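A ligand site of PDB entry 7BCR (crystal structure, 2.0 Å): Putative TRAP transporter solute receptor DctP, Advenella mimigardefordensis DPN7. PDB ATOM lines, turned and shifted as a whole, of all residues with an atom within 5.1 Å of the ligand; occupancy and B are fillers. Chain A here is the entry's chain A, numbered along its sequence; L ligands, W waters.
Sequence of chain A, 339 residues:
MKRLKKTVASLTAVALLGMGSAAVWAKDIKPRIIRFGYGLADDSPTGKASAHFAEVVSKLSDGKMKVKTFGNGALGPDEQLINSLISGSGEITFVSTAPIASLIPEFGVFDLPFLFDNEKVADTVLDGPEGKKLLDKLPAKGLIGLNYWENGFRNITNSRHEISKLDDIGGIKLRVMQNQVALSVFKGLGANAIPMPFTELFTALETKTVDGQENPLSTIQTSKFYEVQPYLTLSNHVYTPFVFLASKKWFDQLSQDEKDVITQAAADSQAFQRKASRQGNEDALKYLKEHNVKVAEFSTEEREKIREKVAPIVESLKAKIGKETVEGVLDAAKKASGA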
ATOM      1  N   TYR A  38      26.072 -23.546 -10.349  1.00  0.00           N
ATOM      2  CA  TYR A  38      25.884 -24.120 -11.670  1.00  0.00           C
ATOM      3  C   TYR A  38      27.173 -24.031 -12.479  1.00  0.00           C
ATOM      4  O   TYR A  38      28.150 -23.373 -12.091  1.00  0.00           O
ATOM      5  CB  TYR A  38      24.711 -23.451 -12.440  1.00  0.00           C
ATOM      6  CG  TYR A  38      24.855 -21.960 -12.630  1.00  0.00           C
ATOM      7  CD1 TYR A  38      24.303 -21.074 -11.736  1.00  0.00           C
ATOM      8  CD2 TYR A  38      25.512 -21.434 -13.752  1.00  0.00           C
ATOM      9  CE1 TYR A  38      24.406 -19.706 -11.894  1.00  0.00           C
ATOM     10  CE2 TYR A  38      25.628 -20.067 -13.917  1.00  0.00           C
ATOM     11  CZ  TYR A  38      25.075 -19.205 -13.004  1.00  0.00           C
ATOM     12  OH  TYR A  38      25.210 -17.837 -13.193  1.00  0.00           O
ATOM     13  N   GLY A  39      27.160 -24.761 -13.578  1.00  0.00           N
ATOM     14  CA  GLY A  39      28.375 -24.953 -14.367  1.00  0.00           C
ATOM     15  C   GLY A  39      28.684 -23.926 -15.431  1.00  0.00           C
ATOM     16  O   GLY A  39      29.865 -23.588 -15.633  1.00  0.00           O
ATOM     17  N   LEU A  40      27.660 -23.486 -16.161  1.00  0.00           N
ATOM     18  CA  LEU A  40      27.859 -22.539 -17.247  1.00  0.00           C
ATOM     19  C   LEU A  40      28.322 -21.171 -16.720  1.00  0.00           C
ATOM     20  O   LEU A  40      28.206 -20.858 -15.543  1.00  0.00           O
ATOM     21  CB  LEU A  40      26.563 -22.362 -18.032  1.00  0.00           C
ATOM     22  CG  LEU A  40      25.972 -23.589 -18.744  1.00  0.00           C
ATOM     23  CD1 LEU A  40      24.747 -23.151 -19.553  1.00  0.00           C
ATOM     24  CD2 LEU A  40      26.983 -24.237 -19.663  1.00  0.00           C
ATOM     25  N   ASP A  78      28.324 -30.618 -12.639  1.00  0.00           N
ATOM     26  CA  ASP A  78      26.981 -31.168 -12.433  1.00  0.00           C
ATOM     27  C   ASP A  78      26.987 -32.312 -11.410  1.00  0.00           C
ATOM     28  O   ASP A  78      26.121 -32.393 -10.530  1.00  0.00           O
ATOM     29  CB  ASP A  78      26.436 -31.691 -13.760  1.00  0.00           C
ATOM     30  CG  ASP A  78      25.994 -30.586 -14.690  1.00  0.00           C
ATOM     31  OD1 ASP A  78      26.118 -29.401 -14.311  1.00  0.00           O
ATOM     32  OD2 ASP A  78      25.487 -30.905 -15.780  1.00  0.00           O
ATOM     33  N   PHE A  94      20.674 -26.249 -11.747  1.00  0.00           N
ATOM     34  CA  PHE A  94      20.219 -26.865 -12.996  1.00  0.00           C
ATOM     35  C   PHE A  94      21.390 -27.692 -13.517  1.00  0.00           C
ATOM     36  O   PHE A  94      22.552 -27.301 -13.394  1.00  0.00           O
ATOM     37  CB  PHE A  94      19.752 -25.829 -14.022  1.00  0.00           C
ATOM     38  CG  PHE A  94      20.852 -24.968 -14.555  1.00  0.00           C
ATOM     39  CD1 PHE A  94      21.662 -25.404 -15.591  1.00  0.00           C
ATOM     40  CD2 PHE A  94      21.072 -23.700 -13.996  1.00  0.00           C
ATOM     41  CE1 PHE A  94      22.700 -24.599 -16.048  1.00  0.00           C
ATOM     42  CE2 PHE A  94      22.098 -22.898 -14.480  1.00  0.00           C
ATOM     43  CZ  PHE A  94      22.897 -23.356 -15.502  1.00  0.00           C
ATOM     44  N   VAL A  95      21.080 -28.874 -14.013  1.00  0.00           N
ATOM     45  CA  VAL A  95      22.098 -29.775 -14.551  1.00  0.00           C
ATOM     46  C   VAL A  95      21.543 -30.367 -15.837  1.00  0.00           C
ATOM     47  O   VAL A  95      20.321 -30.410 -16.047  1.00  0.00           O
ATOM     48  CB  VAL A  95      22.486 -30.914 -13.614  1.00  0.00           C
ATOM     49  CG1 VAL A  95      23.176 -30.353 -12.387  1.00  0.00           C
ATOM     50  CG2 VAL A  95      21.251 -31.766 -13.275  1.00  0.00           C
ATOM     51  N   SER A  96      22.451 -30.836 -16.686  1.00  0.00           N
ATOM     52  CA  SER A  96      22.019 -31.605 -17.860  1.00  0.00           C
ATOM     53  C   SER A  96      21.471 -32.958 -17.399  1.00  0.00           C
ATOM     54  O   SER A  96      21.775 -33.442 -16.312  1.00  0.00           O
ATOM     55  CB  SER A  96      23.178 -31.780 -18.842  1.00  0.00           C
ATOM     56  OG  SER A  96      23.400 -30.590 -19.562  1.00  0.00           O
ATOM     57  N   ASN A 151      18.894 -26.742 -22.291  1.00  0.00           N
ATOM     58  CA  ASN A 151      20.304 -26.617 -22.602  1.00  0.00           C
ATOM     59  C   ASN A 151      20.446 -26.345 -24.093  1.00  0.00           C
ATOM     60  O   ASN A 151      20.857 -25.240 -24.489  1.00  0.00           O
ATOM     61  CB  ASN A 151      21.049 -27.883 -22.158  1.00  0.00           C
ATOM     62  CG  ASN A 151      22.556 -27.719 -22.230  1.00  0.00           C
ATOM     63  OD1 ASN A 151      23.038 -26.766 -22.802  1.00  0.00           O
ATOM     64  ND2 ASN A 151      23.281 -28.651 -21.631  1.00  0.00           N
ATOM     65  N   ARG A 154      22.912 -29.625 -29.637  1.00  0.00           N
ATOM     66  CA  ARG A 154      24.358 -29.645 -29.455  1.00  0.00           C
ATOM     67  C   ARG A 154      25.072 -29.716 -30.795  1.00  0.00           C
ATOM     68  O   ARG A 154      24.605 -30.394 -31.721  1.00  0.00           O
ATOM     69  CB  ARG A 154      24.802 -30.842 -28.590  1.00  0.00           C
ATOM     70  CG  ARG A 154      24.010 -30.982 -27.265  1.00  0.00           C
ATOM     71  CD  ARG A 154      24.434 -32.245 -26.568  1.00  0.00           C
ATOM     72  NE  ARG A 154      25.771 -32.124 -25.966  1.00  0.00           N
ATOM     73  CZ  ARG A 154      25.994 -31.626 -24.759  1.00  0.00           C
ATOM     74  NH1 ARG A 154      24.979 -31.161 -24.007  1.00  0.00           N
ATOM     75  NH2 ARG A 154      27.232 -31.602 -24.307  1.00  0.00           N
ATOM     76  N   ARG A 175      35.579 -35.093 -26.465  1.00  0.00           N
ATOM     77  CA  ARG A 175      34.962 -35.116 -25.152  1.00  0.00           C
ATOM     78  C   ARG A 175      33.456 -35.290 -25.298  1.00  0.00           C
ATOM     79  O   ARG A 175      32.808 -34.592 -26.082  1.00  0.00           O
ATOM     80  CB  ARG A 175      35.255 -33.819 -24.388  1.00  0.00           C
ATOM     81  CG  ARG A 175      34.688 -33.816 -22.987  1.00  0.00           C
ATOM     82  CD  ARG A 175      33.345 -33.132 -22.954  1.00  0.00           C
ATOM     83  NE  ARG A 175      32.702 -33.171 -21.643  1.00  0.00           N
ATOM     84  CZ  ARG A 175      31.542 -32.563 -21.385  1.00  0.00           C
ATOM     85  NH1 ARG A 175      30.916 -31.915 -22.351  1.00  0.00           N
ATOM     86  NH2 ARG A 175      30.985 -32.646 -20.186  1.00  0.00           N
ATOM     87  N   MET A 177      29.800 -36.039 -22.546  1.00  0.00           N
ATOM     88  CA  MET A 177      29.191 -36.088 -21.212  1.00  0.00           C
ATOM     89  C   MET A 177      29.323 -37.503 -20.652  1.00  0.00           C
ATOM     90  O   MET A 177      29.563 -38.488 -21.359  1.00  0.00           O
ATOM     91  CB  MET A 177      27.745 -35.625 -21.283  1.00  0.00           C
ATOM     92  CG  MET A 177      27.592 -34.147 -21.626  1.00  0.00           C
ATOM     93  SD  MET A 177      25.964 -33.444 -21.400  1.00  0.00           S
ATOM     94  CE  MET A 177      25.042 -34.290 -22.714  1.00  0.00           C
ATOM     95  N   PHE A 198      32.269 -31.067 -17.353  1.00  0.00           N
ATOM     96  CA  PHE A 198      32.314 -29.805 -18.079  1.00  0.00           C
ATOM     97  C   PHE A 198      33.353 -28.832 -17.505  1.00  0.00           C
ATOM     98  O   PHE A 198      33.919 -28.015 -18.246  1.00  0.00           O
ATOM     99  CB  PHE A 198      30.935 -29.177 -18.046  1.00  0.00           C
ATOM    100  CG  PHE A 198      30.813 -27.894 -18.837  1.00  0.00           C
ATOM    101  CD1 PHE A 198      30.668 -27.926 -20.222  1.00  0.00           C
ATOM    102  CD2 PHE A 198      30.822 -26.682 -18.186  1.00  0.00           C
ATOM    103  CE1 PHE A 198      30.555 -26.763 -20.938  1.00  0.00           C
ATOM    104  CE2 PHE A 198      30.679 -25.504 -18.901  1.00  0.00           C
ATOM    105  CZ  PHE A 198      30.562 -25.542 -20.275  1.00  0.00           C
ATOM    106  N   GLU A 214      31.132 -31.167 -28.022  1.00  0.00           N
ATOM    107  CA  GLU A 214      29.825 -30.827 -28.584  1.00  0.00           C
ATOM    108  C   GLU A 214      28.915 -30.209 -27.542  1.00  0.00           C
ATOM    109  O   GLU A 214      28.760 -30.764 -26.440  1.00  0.00           O
ATOM    110  CB  GLU A 214      29.202 -32.112 -29.185  1.00  0.00           C
ATOM    111  CG  GLU A 214      29.175 -33.317 -28.292  1.00  0.00           C
ATOM    112  CD  GLU A 214      27.811 -33.456 -27.639  1.00  0.00           C
ATOM    113  OE1 GLU A 214      26.790 -33.303 -28.329  1.00  0.00           O
ATOM    114  OE2 GLU A 214      27.798 -33.636 -26.410  1.00  0.00           O
ATOM    115  N   ASN A 215      28.441 -29.006 -27.843  1.00  0.00           N
ATOM    116  CA  ASN A 215      27.589 -28.273 -26.914  1.00  0.00           C
ATOM    117  C   ASN A 215      26.720 -27.342 -27.745  1.00  0.00           C
ATOM    118  O   ASN A 215      26.927 -27.221 -28.948  1.00  0.00           O
ATOM    119  CB  ASN A 215      28.419 -27.470 -25.882  1.00  0.00           C
ATOM    120  CG  ASN A 215      28.611 -28.217 -24.570  1.00  0.00           C
ATOM    121  OD1 ASN A 215      27.651 -28.436 -23.853  1.00  0.00           O
ATOM    122  ND2 ASN A 215      29.839 -28.605 -24.274  1.00  0.00           N
ATOM    123  N   PRO A 216      25.753 -26.652 -27.128  1.00  0.00           N
ATOM    124  CA  PRO A 216      25.013 -25.628 -27.863  1.00  0.00           C
ATOM    125  C   PRO A 216      25.860 -24.406 -28.123  1.00  0.00           C
ATOM    126  O   PRO A 216      26.854 -24.139 -27.443  1.00  0.00           O
ATOM    127  CB  PRO A 216      23.817 -25.295 -26.972  1.00  0.00           C
ATOM    128  CG  PRO A 216      23.722 -26.511 -26.020  1.00  0.00           C
ATOM    129  CD  PRO A 216      25.134 -26.963 -25.821  1.00  0.00           C
ATOM    130  N   THR A 219      26.793 -21.883 -25.381  1.00  0.00           N
ATOM    131  CA  THR A 219      27.825 -22.363 -24.459  1.00  0.00           C
ATOM    132  C   THR A 219      29.202 -22.318 -25.119  1.00  0.00           C
ATOM    133  O   THR A 219      30.189 -21.936 -24.492  1.00  0.00           O
ATOM    134  CB  THR A 219      27.489 -23.792 -24.000  1.00  0.00           C
ATOM    135  OG1 THR A 219      26.189 -23.772 -23.420  1.00  0.00           O
ATOM    136  CG2 THR A 219      28.558 -24.313 -23.058  1.00  0.00           C
ATOM    137  N   PHE A 242      17.870 -29.408 -19.547  1.00  0.00           N
ATOM    138  CA  PHE A 242      18.317 -29.228 -18.174  1.00  0.00           C
ATOM    139  C   PHE A 242      17.162 -29.677 -17.283  1.00  0.00           C
ATOM    140  O   PHE A 242      15.989 -29.540 -17.656  1.00  0.00           O
ATOM    141  CB  PHE A 242      18.636 -27.771 -17.823  1.00  0.00           C
ATOM    142  CG  PHE A 242      19.978 -27.247 -18.369  1.00  0.00           C
ATOM    143  CD1 PHE A 242      21.145 -27.954 -18.236  1.00  0.00           C
ATOM    144  CD2 PHE A 242      20.023 -26.005 -18.990  1.00  0.00           C
ATOM    145  CE1 PHE A 242      22.361 -27.443 -18.715  1.00  0.00           C
ATOM    146  CE2 PHE A 242      21.202 -25.503 -19.495  1.00  0.00           C
ATOM    147  CZ  PHE A 242      22.383 -26.208 -19.335  1.00  0.00           C
HETATM  148  O1  LIG L   1      28.505 -30.389 -21.862  1.00  0.00           O
HETATM  149  C1  LIG L   1      27.889 -30.524 -20.716  1.00  0.00           C
HETATM  150  O2  LIG L   1      28.339 -31.247 -19.797  1.00  0.00           O
HETATM  151  C2  LIG L   1      26.567 -29.839 -20.501  1.00  0.00           C
HETATM  152  O3  LIG L   1      26.186 -29.519 -21.846  1.00  0.00           O
HETATM  153  C3  LIG L   1      26.592 -28.618 -19.593  1.00  0.00           C
HETATM  154  O4  LIG L   1      27.834 -28.015 -19.724  1.00  0.00           O
HETATM  155  C4  LIG L   1      26.413 -29.024 -18.178  1.00  0.00           C
HETATM  156  O5  LIG L   1      25.147 -29.726 -18.102  1.00  0.00           O
HETATM  157  C5  LIG L   1      26.216 -28.036 -17.053  1.00  0.00           C
HETATM  158  O6  LIG L   1      27.371 -27.960 -16.279  1.00  0.00           O
HETATM  159  C6  LIG L   1      25.800 -26.670 -17.494  1.00  0.00           C
HETATM  160  O7  LIG L   1      25.601 -25.827 -16.367  1.00  0.00           O
HETATM  161  O   HOH W   1      29.102 -29.735 -15.195  1.00  0.00           O
HETATM  162  O   HOH W   2      25.193 -26.762 -13.811  1.00  0.00           O
HETATM  163  O   HOH W   3      27.622 -32.490 -17.611  1.00  0.00           O
HETATM  164  O   HOH W   4      25.644 -26.163 -22.368  1.00  0.00           O
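N of Ser 96 sits close to O5 of the ligand, 3.2 Å away.
OG of Ser 96 sits at hydrogen-bond distance from O5 of the ligand (2.4 Å).
The side-chain carboxylate of Asp 78 sits at hydrogen-bond distance from an oxygen (O5) of the ligand (2.6 Å).
An oxygen (O3) of the ligand is in hydrogen-bond range of the side-chain amide oxygen (OD1) of Asn 215 (2.7 Å).
NH1 of Arg 175 lies within salt-bridge range of O1 of the ligand, at 2.9 Å.
An oxygen (O1) of the ligand is in salt-bridge range of the guanidinium group (NH2) of Arg 154 (3.0 Å).
ND2 of Asn 151 sits at hydrogen-bond distance from O3 of the ligand (3.0 Å).
N of Leu 40 is in hydrogen-bond range of O7 of the ligand (3.1 Å).
An oxygen (O7) of the ligand sits at hydrogen-bond distance from the backbone NH (N) of Gly 39 (3.4 Å).
The backbone NH (N) of Ser 96 lies within hydrogen-bond range of the side-chain carboxylate (OD2) of Asp 78 (3.2 Å).
OG of Ser 96 sits at hydrogen-bond distance from ND2 of Asn 151, 2.8 Å away.
OD1 of Asn 215 sits at hydrogen-bond distance from NH2 of Arg 154 (3.2 Å).
NH1 of Arg 154 sits close to SD of Met 177 (3.6 Å).
NE of Arg 154 is in salt-bridge range of OE2 of Glu 214.
SD of Met 177 lies close to O2 of the ligand (3.6 Å).
Residues that only touch the ligand: Phe 94 (3.2 Å), Phe 198 (2.9 Å) and Phe 242 (3.7 Å).
Hydrophobic or aromatic side chains within 4 Å of the ligand: Leu 40, Phe 94, Met 177, Phe 198 and Phe 242.
12 residues have an atom within 4 Å of the ligand: Gly 39, Leu 40, Asp 78, Phe 94, Ser 96, Asn 151, Arg 154, Arg 175, Met 177, Phe 198, Asn 215 and Phe 242.
Water W3 lies within hydrogen-bond range of an oxygen (O2) of the ligand (2.6 Å) and the side-chain carboxylate (OD2) of Asp 78 (3.2 Å).
Water W1 bridges O6 of the ligand (2.7 Å) and N of Asp 78 (2.8 Å).
Water W2 lies within hydrogen-bond range of O of Phe 94, O7 of the ligand, N of Gly 39 and OD1 of Asp 78.
Water W4 lies within hydrogen-bond range of the side-chain hydroxyl (OG1) of Thr 219, the side-chain amide oxygen (OD1) of Asn 151, the side-chain amide oxygen (OD1) of Asn 215 and an oxygen (O3) of the ligand.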
